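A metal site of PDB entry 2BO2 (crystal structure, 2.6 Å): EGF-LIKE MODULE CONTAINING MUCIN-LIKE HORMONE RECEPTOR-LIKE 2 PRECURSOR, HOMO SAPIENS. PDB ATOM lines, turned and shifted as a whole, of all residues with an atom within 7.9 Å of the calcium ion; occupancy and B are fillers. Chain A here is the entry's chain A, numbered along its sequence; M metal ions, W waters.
The calcium ion is bound by the side-chain carboxylate (OD1) of Asp 95, the side-chain amide oxygen (OD1) of Asn 114, the backbone carbonyl oxygen (O) of Val 96, the backbone carbonyl oxygen (O) of Thr 115, the backbone carbonyl oxygen (O) of Ser 118, water W1 and the side-chain carboxylate (OE2) of Glu 98.
The side-chain hydroxyl (OG) of Ser 118 sits close to the side-chain amino group (NZ) of Lys 138 (3.2 Å).
SG of Cys 99 lies within hydrogen-bond range of N of Asn 114 (3.3 Å).
OD1 of Asp 95 lies close to N of Gly 117.
O of Gly 75 is in hydrogen-bond range of N of Val 96 (3.0 Å).
The side-chain hydroxyl of Thr 115 lies close to the backbone NH of Ser 118, at 3.5 Å.
OG1 of Thr 115 is in hydrogen-bond range of N of Tyr 119 (3.2 Å).
Of the 18 residues printed, 6 come within 4 Å of the calcium ion.
The nearest printed residue that does not touch the calcium ion is Gly 117 (4.02 Å).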
ATOM      1  N   PRO A  74      30.299   9.726  -0.740  1.00  0.00           N
ATOM      2  CA  PRO A  74      30.292  11.159  -0.443  1.00  0.00           C
ATOM      3  C   PRO A  74      28.891  11.721  -0.663  1.00  0.00           C
ATOM      4  O   PRO A  74      28.265  11.491  -1.695  1.00  0.00           O
ATOM      5  CB  PRO A  74      31.264  11.723  -1.485  1.00  0.00           C
ATOM      6  CG  PRO A  74      32.241  10.617  -1.725  1.00  0.00           C
ATOM      7  CD  PRO A  74      31.523   9.309  -1.461  1.00  0.00           C
ATOM      8  N   GLY A  75      28.381  12.437   0.340  1.00  0.00           N
ATOM      9  CA  GLY A  75      27.038  13.010   0.270  1.00  0.00           C
ATOM     10  C   GLY A  75      26.038  12.169   1.071  1.00  0.00           C
ATOM     11  O   GLY A  75      24.872  12.541   1.217  1.00  0.00           O
ATOM     12  N   TYR A  76      26.515  11.048   1.601  1.00  0.00           N
ATOM     13  CA  TYR A  76      25.682  10.155   2.380  1.00  0.00           C
ATOM     14  C   TYR A  76      26.344   9.845   3.730  1.00  0.00           C
ATOM     15  O   TYR A  76      27.566   9.860   3.846  1.00  0.00           O
ATOM     16  CB  TYR A  76      25.408   8.858   1.611  1.00  0.00           C
ATOM     17  CG  TYR A  76      24.859   9.067   0.218  1.00  0.00           C
ATOM     18  CD1 TYR A  76      25.703   9.284  -0.867  1.00  0.00           C
ATOM     19  CD2 TYR A  76      23.494   9.021  -0.030  1.00  0.00           C
ATOM     20  CE1 TYR A  76      25.208   9.470  -2.142  1.00  0.00           C
ATOM     21  CE2 TYR A  76      22.983   9.189  -1.306  1.00  0.00           C
ATOM     22  CZ  TYR A  76      23.850   9.406  -2.353  1.00  0.00           C
ATOM     23  OH  TYR A  76      23.352   9.568  -3.631  1.00  0.00           O
ATOM     24  N   GLN A  94      22.112   7.083   4.593  1.00  0.00           N
ATOM     25  CA  GLN A  94      21.042   7.969   4.155  1.00  0.00           C
ATOM     26  C   GLN A  94      21.699   9.213   3.579  1.00  0.00           C
ATOM     27  O   GLN A  94      22.862   9.496   3.866  1.00  0.00           O
ATOM     28  CB  GLN A  94      20.132   8.329   5.341  1.00  0.00           C
ATOM     29  CG  GLN A  94      18.640   8.141   5.080  1.00  0.00           C
ATOM     30  CD  GLN A  94      18.275   6.713   4.683  1.00  0.00           C
ATOM     31  OE1 GLN A  94      18.156   6.389   3.495  1.00  0.00           O
ATOM     32  NE2 GLN A  94      18.040   5.860   5.685  1.00  0.00           N
ATOM     33  N   ASP A  95      20.958   9.950   2.765  1.00  0.00           N
ATOM     34  CA  ASP A  95      21.473  11.182   2.173  1.00  0.00           C
ATOM     35  C   ASP A  95      21.560  12.277   3.219  1.00  0.00           C
ATOM     36  O   ASP A  95      20.773  12.311   4.166  1.00  0.00           O
ATOM     37  CB  ASP A  95      20.573  11.629   1.009  1.00  0.00           C
ATOM     38  CG  ASP A  95      20.639  13.126   0.763  1.00  0.00           C
ATOM     39  OD1 ASP A  95      21.587  13.582   0.100  1.00  0.00           O
ATOM     40  OD2 ASP A  95      19.715  13.842   1.203  1.00  0.00           O
ATOM     41  N   VAL A  96      22.540  13.161   3.064  1.00  0.00           N
ATOM     42  CA  VAL A  96      22.713  14.288   3.970  1.00  0.00           C
ATOM     43  C   VAL A  96      22.038  15.523   3.380  1.00  0.00           C
ATOM     44  O   VAL A  96      22.260  15.863   2.217  1.00  0.00           O
ATOM     45  CB  VAL A  96      24.213  14.611   4.172  1.00  0.00           C
ATOM     46  CG1 VAL A  96      24.400  16.064   4.527  1.00  0.00           C
ATOM     47  CG2 VAL A  96      24.821  13.709   5.217  1.00  0.00           C
ATOM     48  N   ASP A  97      21.190  16.174   4.172  1.00  0.00           N
ATOM     49  CA  ASP A  97      20.527  17.384   3.697  1.00  0.00           C
ATOM     50  C   ASP A  97      21.369  18.606   4.067  1.00  0.00           C
ATOM     51  O   ASP A  97      21.236  19.156   5.156  1.00  0.00           O
ATOM     52  CB  ASP A  97      19.132  17.515   4.305  1.00  0.00           C
ATOM     53  CG  ASP A  97      18.331  18.633   3.660  1.00  0.00           C
ATOM     54  OD1 ASP A  97      18.912  19.693   3.366  1.00  0.00           O
ATOM     55  OD2 ASP A  97      17.119  18.439   3.437  1.00  0.00           O
ATOM     56  N   GLU A  98      22.244  18.991   3.158  1.00  0.00           N
ATOM     57  CA  GLU A  98      23.159  20.105   3.384  1.00  0.00           C
ATOM     58  C   GLU A  98      22.426  21.404   3.674  1.00  0.00           C
ATOM     59  O   GLU A  98      22.964  22.298   4.331  1.00  0.00           O
ATOM     60  CB  GLU A  98      24.112  20.279   2.198  1.00  0.00           C
ATOM     61  CG  GLU A  98      25.104  19.147   2.013  1.00  0.00           C
ATOM     62  CD  GLU A  98      24.556  18.008   1.183  1.00  0.00           C
ATOM     63  OE1 GLU A  98      25.347  17.126   0.787  1.00  0.00           O
ATOM     64  OE2 GLU A  98      23.335  17.995   0.917  1.00  0.00           O
ATOM     65  N   CYS A  99      21.199  21.532   3.165  1.00  0.00           N
ATOM     66  CA  CYS A  99      20.432  22.761   3.363  1.00  0.00           C
ATOM     67  C   CYS A  99      19.891  22.904   4.778  1.00  0.00           C
ATOM     68  O   CYS A  99      20.112  23.921   5.421  1.00  0.00           O
ATOM     69  CB  CYS A  99      19.306  22.875   2.336  1.00  0.00           C
ATOM     70  SG  CYS A  99      19.796  22.606   0.596  1.00  0.00           S
ATOM     71  N   PHE A 113      19.266  24.139  -2.358  1.00  0.00           N
ATOM     72  CA  PHE A 113      18.317  23.113  -2.780  1.00  0.00           C
ATOM     73  C   PHE A 113      18.971  21.753  -2.643  1.00  0.00           C
ATOM     74  O   PHE A 113      20.005  21.487  -3.272  1.00  0.00           O
ATOM     75  CB  PHE A 113      17.860  23.336  -4.218  1.00  0.00           C
ATOM     76  CG  PHE A 113      16.825  22.348  -4.680  1.00  0.00           C
ATOM     77  CD1 PHE A 113      15.477  22.594  -4.468  1.00  0.00           C
ATOM     78  CD2 PHE A 113      17.213  21.149  -5.257  1.00  0.00           C
ATOM     79  CE1 PHE A 113      14.523  21.652  -4.827  1.00  0.00           C
ATOM     80  CE2 PHE A 113      16.263  20.199  -5.621  1.00  0.00           C
ATOM     81  CZ  PHE A 113      14.921  20.456  -5.402  1.00  0.00           C
ATOM     82  N   ASN A 114      18.411  20.898  -1.801  1.00  0.00           N
ATOM     83  CA  ASN A 114      18.996  19.578  -1.550  1.00  0.00           C
ATOM     84  C   ASN A 114      18.674  18.512  -2.580  1.00  0.00           C
ATOM     85  O   ASN A 114      17.537  18.383  -3.029  1.00  0.00           O
ATOM     86  CB  ASN A 114      18.635  19.075  -0.143  1.00  0.00           C
ATOM     87  CG  ASN A 114      19.283  17.747   0.166  1.00  0.00           C
ATOM     88  OD1 ASN A 114      20.496  17.587   0.069  1.00  0.00           O
ATOM     89  ND2 ASN A 114      18.457  16.763   0.515  1.00  0.00           N
ATOM     90  N   THR A 115      19.684  17.704  -2.907  1.00  0.00           N
ATOM     91  CA  THR A 115      19.540  16.601  -3.832  1.00  0.00           C
ATOM     92  C   THR A 115      20.195  15.350  -3.230  1.00  0.00           C
ATOM     93  O   THR A 115      20.960  15.447  -2.271  1.00  0.00           O
ATOM     94  CB  THR A 115      20.212  16.892  -5.186  1.00  0.00           C
ATOM     95  OG1 THR A 115      21.631  16.753  -5.047  1.00  0.00           O
ATOM     96  CG2 THR A 115      19.893  18.307  -5.645  1.00  0.00           C
ATOM     97  N   VAL A 116      19.904  14.199  -3.818  1.00  0.00           N
ATOM     98  CA  VAL A 116      20.468  12.934  -3.359  1.00  0.00           C
ATOM     99  C   VAL A 116      21.953  12.822  -3.727  1.00  0.00           C
ATOM    100  O   VAL A 116      22.311  12.760  -4.904  1.00  0.00           O
ATOM    101  CB  VAL A 116      19.719  11.736  -3.978  1.00  0.00           C
ATOM    102  CG1 VAL A 116      19.565  10.612  -2.960  1.00  0.00           C
ATOM    103  CG2 VAL A 116      18.354  12.183  -4.501  1.00  0.00           C
ATOM    104  N   GLY A 117      22.818  12.782  -2.716  1.00  0.00           N
ATOM    105  CA  GLY A 117      24.244  12.653  -2.946  1.00  0.00           C
ATOM    106  C   GLY A 117      24.931  14.009  -3.042  1.00  0.00           C
ATOM    107  O   GLY A 117      26.136  14.114  -2.861  1.00  0.00           O
ATOM    108  N   SER A 118      24.150  15.047  -3.347  1.00  0.00           N
ATOM    109  CA  SER A 118      24.704  16.386  -3.486  1.00  0.00           C
ATOM    110  C   SER A 118      23.712  17.440  -3.020  1.00  0.00           C
ATOM    111  O   SER A 118      22.869  17.200  -2.148  1.00  0.00           O
ATOM    112  CB  SER A 118      25.095  16.652  -4.929  1.00  0.00           C
ATOM    113  OG  SER A 118      26.151  17.588  -5.014  1.00  0.00           O
ATOM    114  N   TYR A 119      23.810  18.623  -3.631  1.00  0.00           N
ATOM    115  CA  TYR A 119      22.925  19.734  -3.335  1.00  0.00           C
ATOM    116  C   TYR A 119      23.211  20.862  -4.331  1.00  0.00           C
ATOM    117  O   TYR A 119      24.282  20.909  -4.943  1.00  0.00           O
ATOM    118  CB  TYR A 119      23.112  20.225  -1.900  1.00  0.00           C
ATOM    119  CG  TYR A 119      24.332  21.087  -1.680  1.00  0.00           C
ATOM    120  CD1 TYR A 119      24.311  22.445  -1.981  1.00  0.00           C
ATOM    121  CD2 TYR A 119      25.481  20.566  -1.098  1.00  0.00           C
ATOM    122  CE1 TYR A 119      25.415  23.249  -1.743  1.00  0.00           C
ATOM    123  CE2 TYR A 119      26.584  21.365  -0.852  1.00  0.00           C
ATOM    124  CZ  TYR A 119      26.546  22.696  -1.182  1.00  0.00           C
ATOM    125  OH  TYR A 119      27.653  23.492  -0.950  1.00  0.00           O
ATOM    126  N   SER A 120      22.238  21.760  -4.510  1.00  0.00           N
ATOM    127  CA  SER A 120      22.412  22.859  -5.449  1.00  0.00           C
ATOM    128  C   SER A 120      21.937  24.182  -4.872  1.00  0.00           C
ATOM    129  O   SER A 120      21.008  24.223  -4.057  1.00  0.00           O
ATOM    130  CB  SER A 120      21.673  22.566  -6.748  1.00  0.00           C
ATOM    131  OG  SER A 120      20.290  22.345  -6.518  1.00  0.00           O
ATOM    132  N   LYS A 138      26.516  24.621  -7.149  1.00  0.00           N
ATOM    133  CA  LYS A 138      27.135  24.894  -5.857  1.00  0.00           C
ATOM    134  C   LYS A 138      27.989  26.165  -5.879  1.00  0.00           C
ATOM    135  O   LYS A 138      28.348  26.690  -4.824  1.00  0.00           O
ATOM    136  CB  LYS A 138      27.979  23.695  -5.401  1.00  0.00           C
ATOM    137  CG  LYS A 138      27.179  22.417  -5.181  1.00  0.00           C
ATOM    138  CD  LYS A 138      27.770  21.586  -4.059  1.00  0.00           C
ATOM    139  CE  LYS A 138      27.532  20.098  -4.286  1.00  0.00           C
ATOM    140  NZ  LYS A 138      28.313  19.259  -3.333  1.00  0.00           N
HETATM  141 CA    CA M   1      22.074  15.806  -0.171  1.00  0.00          CA
HETATM  142  O   HOH W   1      24.469  14.723   0.142  1.00  0.00           O
